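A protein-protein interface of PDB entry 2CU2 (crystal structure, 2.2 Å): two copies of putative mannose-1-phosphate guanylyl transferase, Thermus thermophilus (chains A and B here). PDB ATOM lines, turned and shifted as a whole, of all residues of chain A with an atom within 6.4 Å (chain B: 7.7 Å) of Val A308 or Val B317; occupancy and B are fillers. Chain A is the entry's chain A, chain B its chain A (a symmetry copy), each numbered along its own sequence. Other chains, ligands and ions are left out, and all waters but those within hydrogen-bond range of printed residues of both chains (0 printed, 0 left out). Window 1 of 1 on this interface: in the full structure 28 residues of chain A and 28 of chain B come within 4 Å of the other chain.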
ATOM      1  N   THR A 286       8.430 -13.682 -10.633  1.00  0.00           N
ATOM      2  CA  THR A 286       8.332 -12.342 -11.193  1.00  0.00           C
ATOM      3  C   THR A 286       8.776 -11.288 -10.180  1.00  0.00           C
ATOM      4  O   THR A 286       8.413 -11.328  -9.011  1.00  0.00           O
ATOM      5  CB  THR A 286       6.873 -12.102 -11.585  1.00  0.00           C
ATOM      6  OG1 THR A 286       6.527 -12.964 -12.669  1.00  0.00           O
ATOM      7  CG2 THR A 286       6.679 -10.652 -12.028  1.00  0.00           C
ATOM      8  N   CYS A 289       7.898  -5.715 -10.982  1.00  0.00           N
ATOM      9  CA  CYS A 289       6.913  -5.362 -12.000  1.00  0.00           C
ATOM     10  C   CYS A 289       5.775  -4.465 -11.523  1.00  0.00           C
ATOM     11  O   CYS A 289       5.544  -4.301 -10.328  1.00  0.00           O
ATOM     12  CB  CYS A 289       6.309  -6.631 -12.608  1.00  0.00           C
ATOM     13  SG  CYS A 289       7.422  -7.529 -13.698  1.00  0.00           S
ATOM     14  N   VAL A 290       5.078  -3.874 -12.487  1.00  0.00           N
ATOM     15  CA  VAL A 290       3.926  -3.029 -12.213  1.00  0.00           C
ATOM     16  C   VAL A 290       2.805  -3.659 -13.031  1.00  0.00           C
ATOM     17  O   VAL A 290       2.886  -3.722 -14.261  1.00  0.00           O
ATOM     18  CB  VAL A 290       4.146  -1.577 -12.687  1.00  0.00           C
ATOM     19  CG1 VAL A 290       2.845  -0.816 -12.609  1.00  0.00           C
ATOM     20  CG2 VAL A 290       5.208  -0.895 -11.825  1.00  0.00           C
ATOM     21  N   VAL A 291       1.770  -4.129 -12.346  1.00  0.00           N
ATOM     22  CA  VAL A 291       0.650  -4.784 -13.003  1.00  0.00           C
ATOM     23  C   VAL A 291      -0.695  -4.115 -12.749  1.00  0.00           C
ATOM     24  O   VAL A 291      -1.058  -3.838 -11.604  1.00  0.00           O
ATOM     25  CB  VAL A 291       0.524  -6.249 -12.528  1.00  0.00           C
ATOM     26  CG1 VAL A 291      -0.682  -6.906 -13.173  1.00  0.00           C
ATOM     27  CG2 VAL A 291       1.803  -7.015 -12.838  1.00  0.00           C
ATOM     28  N   TYR A 292      -1.429  -3.852 -13.821  1.00  0.00           N
ATOM     29  CA  TYR A 292      -2.758  -3.286 -13.693  1.00  0.00           C
ATOM     30  C   TYR A 292      -3.708  -4.258 -14.380  1.00  0.00           C
ATOM     31  O   TYR A 292      -3.569  -4.537 -15.566  1.00  0.00           O
ATOM     32  CB  TYR A 292      -2.878  -1.918 -14.367  1.00  0.00           C
ATOM     33  CG  TYR A 292      -4.192  -1.242 -14.032  1.00  0.00           C
ATOM     34  CD1 TYR A 292      -4.259  -0.267 -13.033  1.00  0.00           C
ATOM     35  CD2 TYR A 292      -5.385  -1.638 -14.650  1.00  0.00           C
ATOM     36  CE1 TYR A 292      -5.475   0.293 -12.655  1.00  0.00           C
ATOM     37  CE2 TYR A 292      -6.619  -1.079 -14.273  1.00  0.00           C
ATOM     38  CZ  TYR A 292      -6.650  -0.114 -13.274  1.00  0.00           C
ATOM     39  OH  TYR A 292      -7.845   0.454 -12.894  1.00  0.00           O
ATOM     40  N   ALA A 293      -4.664  -4.779 -13.625  1.00  0.00           N
ATOM     41  CA  ALA A 293      -5.698  -5.658 -14.146  1.00  0.00           C
ATOM     42  C   ALA A 293      -7.088  -5.179 -13.728  1.00  0.00           C
ATOM     43  O   ALA A 293      -7.517  -5.323 -12.591  1.00  0.00           O
ATOM     44  CB  ALA A 293      -5.444  -7.063 -13.603  1.00  0.00           C
ATOM     45  N   VAL A 298      -4.162 -11.699 -14.629  1.00  0.00           N
ATOM     46  CA  VAL A 298      -2.943 -11.384 -15.361  1.00  0.00           C
ATOM     47  C   VAL A 298      -1.772 -12.242 -14.884  1.00  0.00           C
ATOM     48  O   VAL A 298      -1.388 -12.229 -13.722  1.00  0.00           O
ATOM     49  CB  VAL A 298      -2.620  -9.905 -15.155  1.00  0.00           C
ATOM     50  CG1 VAL A 298      -1.223  -9.601 -15.691  1.00  0.00           C
ATOM     51  CG2 VAL A 298      -3.632  -9.047 -15.890  1.00  0.00           C
ATOM     52  N   ALA A 299      -1.240 -13.155 -15.685  1.00  0.00           N
ATOM     53  CA  ALA A 299      -0.216 -14.056 -15.190  1.00  0.00           C
ATOM     54  C   ALA A 299       1.125 -13.700 -15.804  1.00  0.00           C
ATOM     55  O   ALA A 299       1.248 -13.537 -17.021  1.00  0.00           O
ATOM     56  CB  ALA A 299      -0.577 -15.504 -15.512  1.00  0.00           C
ATOM     57  N   THR A 300       2.127 -13.555 -14.950  1.00  0.00           N
ATOM     58  CA  THR A 300       3.464 -13.237 -15.397  1.00  0.00           C
ATOM     59  C   THR A 300       4.336 -14.389 -14.926  1.00  0.00           C
ATOM     60  O   THR A 300       4.202 -14.870 -13.799  1.00  0.00           O
ATOM     61  CB  THR A 300       3.943 -11.889 -14.825  1.00  0.00           C
ATOM     62  OG1 THR A 300       3.956 -11.940 -13.392  1.00  0.00           O
ATOM     63  CG2 THR A 300       2.998 -10.778 -15.265  1.00  0.00           C
ATOM     64  N   LEU A 301       5.217 -14.838 -15.808  1.00  0.00           N
ATOM     65  CA  LEU A 301       6.079 -15.962 -15.522  1.00  0.00           C
ATOM     66  C   LEU A 301       7.516 -15.646 -15.923  1.00  0.00           C
ATOM     67  O   LEU A 301       7.808 -15.408 -17.101  1.00  0.00           O
ATOM     68  CB  LEU A 301       5.550 -17.176 -16.304  1.00  0.00           C
ATOM     69  CG  LEU A 301       4.077 -17.586 -16.342  1.00  0.00           C
ATOM     70  CD1 LEU A 301       3.832 -18.459 -17.540  1.00  0.00           C
ATOM     71  CD2 LEU A 301       3.706 -18.345 -15.066  1.00  0.00           C
ATOM     72  N   GLY A 302       8.401 -15.622 -14.930  1.00  0.00           N
ATOM     73  CA  GLY A 302       9.813 -15.372 -15.176  1.00  0.00           C
ATOM     74  C   GLY A 302      10.207 -14.058 -15.830  1.00  0.00           C
ATOM     75  O   GLY A 302      11.089 -14.032 -16.689  1.00  0.00           O
ATOM     76  N   VAL A 303       9.569 -12.961 -15.431  1.00  0.00           N
ATOM     77  CA  VAL A 303       9.899 -11.655 -15.992  1.00  0.00           C
ATOM     78  C   VAL A 303      10.169 -10.642 -14.875  1.00  0.00           C
ATOM     79  O   VAL A 303       9.733 -10.826 -13.740  1.00  0.00           O
ATOM     80  CB  VAL A 303       8.758 -11.120 -16.900  1.00  0.00           C
ATOM     81  CG1 VAL A 303       8.681 -11.931 -18.187  1.00  0.00           C
ATOM     82  CG2 VAL A 303       7.435 -11.181 -16.168  1.00  0.00           C
ATOM     83  N   LEU A 306       8.833  -5.155 -15.650  1.00  0.00           N
ATOM     84  CA  LEU A 306       7.864  -4.855 -16.695  1.00  0.00           C
ATOM     85  C   LEU A 306       6.573  -4.222 -16.194  1.00  0.00           C
ATOM     86  O   LEU A 306       6.187  -4.366 -15.030  1.00  0.00           O
ATOM     87  CB  LEU A 306       7.485  -6.122 -17.468  1.00  0.00           C
ATOM     88  CG  LEU A 306       8.488  -6.867 -18.354  1.00  0.00           C
ATOM     89  CD1 LEU A 306       7.764  -8.030 -19.044  1.00  0.00           C
ATOM     90  CD2 LEU A 306       9.065  -5.927 -19.408  1.00  0.00           C
ATOM     91  N   VAL A 307       5.921  -3.502 -17.096  1.00  0.00           N
ATOM     92  CA  VAL A 307       4.626  -2.922 -16.823  1.00  0.00           C
ATOM     93  C   VAL A 307       3.704  -3.752 -17.704  1.00  0.00           C
ATOM     94  O   VAL A 307       3.926  -3.868 -18.906  1.00  0.00           O
ATOM     95  CB  VAL A 307       4.502  -1.443 -17.281  1.00  0.00           C
ATOM     96  CG1 VAL A 307       3.015  -1.047 -17.330  1.00  0.00           C
ATOM     97  CG2 VAL A 307       5.258  -0.520 -16.331  1.00  0.00           C
ATOM     98  N   VAL A 308       2.696  -4.368 -17.103  1.00  0.00           N
ATOM     99  CA  VAL A 308       1.721  -5.143 -17.857  1.00  0.00           C
ATOM    100  C   VAL A 308       0.402  -4.530 -17.407  1.00  0.00           C
ATOM    101  O   VAL A 308       0.033  -4.651 -16.237  1.00  0.00           O
ATOM    102  CB  VAL A 308       1.746  -6.633 -17.478  1.00  0.00           C
ATOM    103  CG1 VAL A 308       0.798  -7.418 -18.396  1.00  0.00           C
ATOM    104  CG2 VAL A 308       3.162  -7.175 -17.584  1.00  0.00           C
ATOM    105  N   ALA A 309      -0.292  -3.853 -18.321  1.00  0.00           N
ATOM    106  CA  ALA A 309      -1.549  -3.194 -17.984  1.00  0.00           C
ATOM    107  C   ALA A 309      -2.684  -3.643 -18.883  1.00  0.00           C
ATOM    108  O   ALA A 309      -2.628  -3.478 -20.104  1.00  0.00           O
ATOM    109  CB  ALA A 309      -1.384  -1.672 -18.072  1.00  0.00           C
ATOM    110  N   LYS A 310      -3.721  -4.200 -18.264  1.00  0.00           N
ATOM    111  CA  LYS A 310      -4.868  -4.713 -19.000  1.00  0.00           C
ATOM    112  C   LYS A 310      -6.156  -3.993 -18.599  1.00  0.00           C
ATOM    113  O   LYS A 310      -6.551  -3.971 -17.441  1.00  0.00           O
ATOM    114  CB  LYS A 310      -4.993  -6.208 -18.707  1.00  0.00           C
ATOM    115  CG  LYS A 310      -6.244  -6.822 -19.340  1.00  0.00           C
ATOM    116  CD  LYS A 310      -7.079  -7.609 -18.328  1.00  0.00           C
ATOM    117  CE  LYS A 310      -8.401  -8.107 -18.919  1.00  0.00           C
ATOM    118  NZ  LYS A 310      -9.327  -6.986 -19.070  1.00  0.00           N
ATOM    119  N   VAL A 315      -4.194  -4.504 -23.970  1.00  0.00           N
ATOM    120  CA  VAL A 315      -3.097  -4.864 -23.089  1.00  0.00           C
ATOM    121  C   VAL A 315      -1.803  -4.176 -23.488  1.00  0.00           C
ATOM    122  O   VAL A 315      -1.468  -4.071 -24.665  1.00  0.00           O
ATOM    123  CB  VAL A 315      -2.853  -6.389 -23.079  1.00  0.00           C
ATOM    124  CG1 VAL A 315      -1.646  -6.716 -22.218  1.00  0.00           C
ATOM    125  CG2 VAL A 315      -4.084  -7.107 -22.539  1.00  0.00           C
ATOM    126  N   LEU A 316      -1.081  -3.711 -22.481  1.00  0.00           N
ATOM    127  CA  LEU A 316       0.193  -3.041 -22.675  1.00  0.00           C
ATOM    128  C   LEU A 316       1.296  -3.829 -21.981  1.00  0.00           C
ATOM    129  O   LEU A 316       1.106  -4.325 -20.873  1.00  0.00           O
ATOM    130  CB  LEU A 316       0.139  -1.632 -22.071  1.00  0.00           C
ATOM    131  CG  LEU A 316       1.488  -0.954 -21.838  1.00  0.00           C
ATOM    132  CD1 LEU A 316       2.157  -0.693 -23.169  1.00  0.00           C
ATOM    133  CD2 LEU A 316       1.299   0.351 -21.070  1.00  0.00           C
ATOM    134  N   VAL A 317       2.442  -3.944 -22.637  1.00  0.00           N
ATOM    135  CA  VAL A 317       3.593  -4.611 -22.046  1.00  0.00           C
ATOM    136  C   VAL A 317       4.807  -3.770 -22.424  1.00  0.00           C
ATOM    137  O   VAL A 317       5.142  -3.656 -23.601  1.00  0.00           O
ATOM    138  CB  VAL A 317       3.777  -6.047 -22.579  1.00  0.00           C
ATOM    139  CG1 VAL A 317       5.050  -6.659 -21.987  1.00  0.00           C
ATOM    140  CG2 VAL A 317       2.576  -6.896 -22.212  1.00  0.00           C
ATOM    141  N   VAL A 318       5.451  -3.170 -21.426  1.00  0.00           N
ATOM    142  CA  VAL A 318       6.619  -2.315 -21.650  1.00  0.00           C
ATOM    143  C   VAL A 318       7.520  -2.289 -20.413  1.00  0.00           C
ATOM    144  O   VAL A 318       7.022  -2.301 -19.294  1.00  0.00           O
ATOM    145  CB  VAL A 318       6.172  -0.852 -21.967  1.00  0.00           C
ATOM    146  CG1 VAL A 318       5.323  -0.313 -20.819  1.00  0.00           C
ATOM    147  CG2 VAL A 318       7.392   0.053 -22.178  1.00  0.00           C
ATOM    148  N   TRP B  17      -2.856 -21.983 -21.975  1.00  0.00           N
ATOM    149  CA  TRP B  17      -3.692 -21.053 -21.217  1.00  0.00           C
ATOM    150  C   TRP B  17      -3.172 -19.673 -21.652  1.00  0.00           C
ATOM    151  O   TRP B  17      -1.973 -19.519 -21.908  1.00  0.00           O
ATOM    152  CB  TRP B  17      -3.456 -21.257 -19.715  1.00  0.00           C
ATOM    153  CG  TRP B  17      -4.253 -20.332 -18.834  1.00  0.00           C
ATOM    154  CD1 TRP B  17      -5.481 -20.578 -18.277  1.00  0.00           C
ATOM    155  CD2 TRP B  17      -3.902 -18.995 -18.456  1.00  0.00           C
ATOM    156  NE1 TRP B  17      -5.914 -19.472 -17.575  1.00  0.00           N
ATOM    157  CE2 TRP B  17      -4.967 -18.487 -17.669  1.00  0.00           C
ATOM    158  CE3 TRP B  17      -2.796 -18.174 -18.708  1.00  0.00           C
ATOM    159  CZ2 TRP B  17      -4.953 -17.191 -17.133  1.00  0.00           C
ATOM    160  CZ3 TRP B  17      -2.783 -16.888 -18.179  1.00  0.00           C
ATOM    161  CH2 TRP B  17      -3.856 -16.409 -17.399  1.00  0.00           C
ATOM    162  N   PRO B  18      -4.042 -18.648 -21.715  1.00  0.00           N
ATOM    163  CA  PRO B  18      -5.476 -18.572 -21.431  1.00  0.00           C
ATOM    164  C   PRO B  18      -6.406 -18.979 -22.569  1.00  0.00           C
ATOM    165  O   PRO B  18      -7.628 -18.918 -22.414  1.00  0.00           O
ATOM    166  CB  PRO B  18      -5.660 -17.108 -21.084  1.00  0.00           C
ATOM    167  CG  PRO B  18      -4.803 -16.465 -22.126  1.00  0.00           C
ATOM    168  CD  PRO B  18      -3.532 -17.313 -22.080  1.00  0.00           C
ATOM    169  N   VAL B 303      10.468  -4.923 -26.065  1.00  0.00           N
ATOM    170  CA  VAL B 303      10.652  -6.243 -25.472  1.00  0.00           C
ATOM    171  C   VAL B 303      11.006  -7.273 -26.549  1.00  0.00           C
ATOM    172  O   VAL B 303      10.728  -7.070 -27.730  1.00  0.00           O
ATOM    173  CB  VAL B 303       9.377  -6.712 -24.718  1.00  0.00           C
ATOM    174  CG1 VAL B 303       9.183  -5.893 -23.448  1.00  0.00           C
ATOM    175  CG2 VAL B 303       8.164  -6.582 -25.611  1.00  0.00           C
ATOM    176  N   LEU B 306       9.284 -12.676 -25.968  1.00  0.00           N
ATOM    177  CA  LEU B 306       8.175 -12.919 -25.056  1.00  0.00           C
ATOM    178  C   LEU B 306       6.925 -13.482 -25.720  1.00  0.00           C
ATOM    179  O   LEU B 306       6.698 -13.322 -26.922  1.00  0.00           O
ATOM    180  CB  LEU B 306       7.771 -11.631 -24.334  1.00  0.00           C
ATOM    181  CG  LEU B 306       8.693 -10.938 -23.325  1.00  0.00           C
ATOM    182  CD1 LEU B 306       7.952  -9.735 -22.728  1.00  0.00           C
ATOM    183  CD2 LEU B 306       9.079 -11.905 -22.209  1.00  0.00           C
ATOM    184  N   VAL B 307       6.125 -14.163 -24.909  1.00  0.00           N
ATOM    185  CA  VAL B 307       4.846 -14.672 -25.347  1.00  0.00           C
ATOM    186  C   VAL B 307       3.866 -13.789 -24.587  1.00  0.00           C
ATOM    187  O   VAL B 307       3.940 -13.682 -23.366  1.00  0.00           O
ATOM    188  CB  VAL B 307       4.584 -16.140 -24.913  1.00  0.00           C
ATOM    189  CG1 VAL B 307       3.083 -16.454 -25.055  1.00  0.00           C
ATOM    190  CG2 VAL B 307       5.403 -17.106 -25.763  1.00  0.00           C
ATOM    191  N   VAL B 308       2.978 -13.121 -25.309  1.00  0.00           N
ATOM    192  CA  VAL B 308       1.959 -12.291 -24.682  1.00  0.00           C
ATOM    193  C   VAL B 308       0.676 -12.832 -25.298  1.00  0.00           C
ATOM    194  O   VAL B 308       0.466 -12.696 -26.505  1.00  0.00           O
ATOM    195  CB  VAL B 308       2.114 -10.806 -25.050  1.00  0.00           C
ATOM    196  CG1 VAL B 308       1.102  -9.967 -24.256  1.00  0.00           C
ATOM    197  CG2 VAL B 308       3.532 -10.342 -24.763  1.00  0.00           C
ATOM    198  N   ALA B 309      -0.164 -13.467 -24.482  1.00  0.00           N
ATOM    199  CA  ALA B 309      -1.402 -14.058 -24.978  1.00  0.00           C
ATOM    200  C   ALA B 309      -2.616 -13.544 -24.228  1.00  0.00           C
ATOM    201  O   ALA B 309      -2.724 -13.707 -23.011  1.00  0.00           O
ATOM    202  CB  ALA B 309      -1.333 -15.586 -24.875  1.00  0.00           C
ATOM    203  N   LYS B 310      -3.533 -12.934 -24.972  1.00  0.00           N
ATOM    204  CA  LYS B 310      -4.735 -12.356 -24.385  1.00  0.00           C
ATOM    205  C   LYS B 310      -6.000 -13.005 -24.949  1.00  0.00           C
ATOM    206  O   LYS B 310      -6.245 -13.010 -26.148  1.00  0.00           O
ATOM    207  CB  LYS B 310      -4.739 -10.857 -24.686  1.00  0.00           C
ATOM    208  CG  LYS B 310      -6.026 -10.173 -24.216  1.00  0.00           C
ATOM    209  CD  LYS B 310      -6.681  -9.345 -25.323  1.00  0.00           C
ATOM    210  CE  LYS B 310      -8.038  -8.773 -24.902  1.00  0.00           C
ATOM    211  NZ  LYS B 310      -9.036  -9.841 -24.874  1.00  0.00           N
ATOM    212  N   VAL B 315      -4.710 -12.584 -19.371  1.00  0.00           N
ATOM    213  CA  VAL B 315      -3.491 -12.287 -20.104  1.00  0.00           C
ATOM    214  C   VAL B 315      -2.298 -13.044 -19.547  1.00  0.00           C
ATOM    215  O   VAL B 315      -2.121 -13.163 -18.337  1.00  0.00           O
ATOM    216  CB  VAL B 315      -3.166 -10.778 -20.078  1.00  0.00           C
ATOM    217  CG1 VAL B 315      -1.843 -10.521 -20.778  1.00  0.00           C
ATOM    218  CG2 VAL B 315      -4.277  -9.996 -20.767  1.00  0.00           C
ATOM    219  N   LEU B 316      -1.481 -13.551 -20.455  1.00  0.00           N
ATOM    220  CA  LEU B 316      -0.280 -14.289 -20.104  1.00  0.00           C
ATOM    221  C   LEU B 316       0.943 -13.566 -20.650  1.00  0.00           C
ATOM    222  O   LEU B 316       0.923 -13.064 -21.772  1.00  0.00           O
ATOM    223  CB  LEU B 316      -0.334 -15.696 -20.714  1.00  0.00           C
ATOM    224  CG  LEU B 316       0.994 -16.447 -20.777  1.00  0.00           C
ATOM    225  CD1 LEU B 316       1.473 -16.740 -19.373  1.00  0.00           C
ATOM    226  CD2 LEU B 316       0.833 -17.743 -21.568  1.00  0.00           C
ATOM    227  N   VAL B 317       2.002 -13.511 -19.853  1.00  0.00           N
ATOM    228  CA  VAL B 317       3.253 -12.910 -20.291  1.00  0.00           C
ATOM    229  C   VAL B 317       4.361 -13.815 -19.765  1.00  0.00           C
ATOM    230  O   VAL B 317       4.537 -13.943 -18.556  1.00  0.00           O
ATOM    231  CB  VAL B 317       3.446 -11.484 -19.734  1.00  0.00           C
ATOM    232  CG1 VAL B 317       4.815 -10.945 -20.158  1.00  0.00           C
ATOM    233  CG2 VAL B 317       2.349 -10.572 -20.248  1.00  0.00           C
ATOM    234  N   VAL B 318       5.092 -14.453 -20.676  1.00  0.00           N
ATOM    235  CA  VAL B 318       6.174 -15.370 -20.308  1.00  0.00           C
ATOM    236  C   VAL B 318       7.221 -15.450 -21.421  1.00  0.00           C
ATOM    237  O   VAL B 318       6.871 -15.414 -22.594  1.00  0.00           O
ATOM    238  CB  VAL B 318       5.611 -16.805 -20.056  1.00  0.00           C
ATOM    239  CG1 VAL B 318       4.887 -17.301 -21.304  1.00  0.00           C
ATOM    240  CG2 VAL B 318       6.743 -17.775 -19.695  1.00  0.00           C
ATOM    241  N   PRO B 319       8.522 -15.530 -21.070  1.00  0.00           N
ATOM    242  CA  PRO B 319       9.510 -15.704 -22.127  1.00  0.00           C
ATOM    243  C   PRO B 319       9.273 -17.003 -22.877  1.00  0.00           C
ATOM    244  O   PRO B 319       8.976 -18.044 -22.304  1.00  0.00           O
ATOM    245  CB  PRO B 319      10.896 -15.736 -21.496  1.00  0.00           C
ATOM    246  CG  PRO B 319      10.775 -15.227 -20.071  1.00  0.00           C
ATOM    247  CD  PRO B 319       9.209 -15.411 -19.794  1.00  0.00           C
ATOM    248  N   LYS B 320       9.390 -16.920 -24.208  1.00  0.00           N
ATOM    249  CA  LYS B 320       8.976 -18.062 -24.993  1.00  0.00           C
ATOM    250  C   LYS B 320       9.762 -19.332 -24.664  1.00  0.00           C
ATOM    251  O   LYS B 320       9.305 -20.441 -24.885  1.00  0.00           O
ATOM    252  CB  LYS B 320       9.045 -17.720 -26.478  1.00  0.00           C
ATOM    253  CG  LYS B 320      10.454 -17.418 -26.977  1.00  0.00           C
ATOM    254  CD  LYS B 320      10.430 -16.867 -28.399  1.00  0.00           C
ATOM    255  CE  LYS B 320      11.818 -16.825 -29.042  1.00  0.00           C
ATOM    256  NZ  LYS B 320      11.789 -15.914 -30.189  1.00  0.00           N
ATOM    257  N   TRP B 322      10.356 -20.367 -21.782  1.00  0.00           N
ATOM    258  CA  TRP B 322       9.758 -21.000 -20.610  1.00  0.00           C
ATOM    259  C   TRP B 322       8.287 -21.371 -20.854  1.00  0.00           C
ATOM    260  O   TRP B 322       7.506 -21.546 -19.927  1.00  0.00           O
ATOM    261  CB  TRP B 322       9.864 -20.025 -19.433  1.00  0.00           C
ATOM    262  CG  TRP B 322      10.085 -20.754 -18.166  1.00  0.00           C
ATOM    263  CD1 TRP B 322      10.716 -22.007 -18.007  1.00  0.00           C
ATOM    264  CD2 TRP B 322       9.736 -20.290 -16.838  1.00  0.00           C
ATOM    265  NE1 TRP B 322      10.805 -22.377 -16.698  1.00  0.00           N
ATOM    266  CE2 TRP B 322      10.169 -21.282 -15.925  1.00  0.00           C
ATOM    267  CE3 TRP B 322       9.100 -19.143 -16.355  1.00  0.00           C
ATOM    268  CZ2 TRP B 322       9.962 -21.107 -14.563  1.00  0.00           C
ATOM    269  CZ3 TRP B 322       8.894 -18.969 -14.992  1.00  0.00           C
ATOM    270  CH2 TRP B 322       9.324 -19.963 -14.094  1.00  0.00           C
ATOM    271  N   VAL B 326       3.838 -22.628 -18.451  1.00  0.00           N
ATOM    272  CA  VAL B 326       2.527 -21.992 -18.457  1.00  0.00           C
ATOM    273  C   VAL B 326       1.496 -22.853 -17.728  1.00  0.00           C
ATOM    274  O   VAL B 326       0.533 -22.340 -17.149  1.00  0.00           O
ATOM    275  CB  VAL B 326       2.032 -21.740 -19.906  1.00  0.00           C
ATOM    276  CG1 VAL B 326       0.581 -21.298 -19.895  1.00  0.00           C
ATOM    277  CG2 VAL B 326       2.899 -20.678 -20.572  1.00  0.00           C
ATOM    278  N   VAL B 329       0.296 -21.921 -14.243  1.00  0.00           N
ATOM    279  CA  VAL B 329      -0.717 -20.888 -14.079  1.00  0.00           C
ATOM    280  C   VAL B 329      -2.070 -21.502 -13.722  1.00  0.00           C
ATOM    281  O   VAL B 329      -2.708 -21.083 -12.753  1.00  0.00           O
ATOM    282  CB  VAL B 329      -0.865 -20.030 -15.371  1.00  0.00           C
ATOM    283  CG1 VAL B 329      -2.042 -19.081 -15.238  1.00  0.00           C
ATOM    284  CG2 VAL B 329       0.415 -19.229 -15.618  1.00  0.00           C
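OG1 of Thr A286 is in hydrogen-bond range of OG1 of Thr A300, at 2.9 Å.
The backbone NH of Lys A310 sits at hydrogen-bond distance from the backbone carbonyl oxygen of Tyr A292, 2.7 Å away.
The backbone carbonyl oxygen of Val A290 is in hydrogen-bond range of the backbone NH of Val A308 (2.9 Å).
O of Val A308 is in hydrogen-bond range of N of Tyr A292, at 2.9 Å.
The backbone carbonyl oxygen (O) of Ala B309 is in hydrogen-bond range of the backbone NH (N) of Leu B316, 2.8 Å away.
O of Val B318 is in hydrogen-bond range of N of Val B307 (2.7 Å).
Of the 17 printed residues of chain B, 11 touch a printed residue of chain A.
Hydrophobic or aromatic side chains of chain B that line the printed part of chain A: Trp B17, Val B308, Val B315, Leu B316, Val B317, Val B318, Pro B319, Trp B322, Val B326 and Val B329.
Of the 21 printed residues of chain A, 10 touch a printed residue of chain B.
Hydrophobic or aromatic side chains of chain A that line the printed part of chain B: Ala A299, Leu A301, Val A303, Val A308, Val A315 and Val A317.
Among the printed residues, 22 pairs touch across the chains.
Among the printed residues, no Asp or Glu carboxylate lies within 4 Å of a Lys or Arg side-chain nitrogen of the other chain.
N of Ala A299 lies within hydrogen-bond range of O of Val B315.
N of Val B317 is in hydrogen-bond range of O of Ala A299 (2.9 Å).
The backbone NH (N) of Leu A301 lies within hydrogen-bond range of the backbone carbonyl oxygen (O) of Val B317 (3.0 Å).
Ala A299 touches Trp B17 (CB to CZ3, 3.7 Å).
O of Ala A299 touches CA of Leu B316 (3.5 Å).
Thr A300 touches Val B317 (CA to O, 3.4 Å).
CD1 of Leu A301 touches CB of Val B318, at 3.5 Å.
O of Leu A301 touches CD of Pro B319, 3.0 Å away.
Trp B322 touches Leu A301 (CZ3 to C, 3.7 Å).
O of Gly A302 touches CG of Pro B319, 3.6 Å away.
CD of Pro B319 touches CG1 of Val A303 (3.9 Å).
Val A308 touches Val B317.
Val B315 touches Lys A310 (CG2 to CG, 3.997 Å).
Val A308 touches Val B317, and with the chains exchanged Val A317 touches Val B308.
Lys A310 touches Val B315, and with the chains exchanged Val A315 touches Lys B310.
Val B315 touches its own counterpart, Val A315.
Val A308 touches one residue of chain B.
Of the printed residues of chain A, Val B317 touches Ala A299 (2.9 Å), Thr A300 (3.4 Å), Leu A301 (3.0 Å) and Val A308 (3.97 Å).
Printed residues of chain A within 4 Å of Val B318: Leu A301 (3.5 Å).
Printed residues of chain A within 4 Å of Trp B322: Leu A301 and Gly A302.
Of the printed residues of chain A, Val B329 touches Ala A299 (3.9 Å) and Leu A301 (3.5 Å).
The nearest printed residue of chain B that does not touch Thr A300 is Val B315 (5.4 Å).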
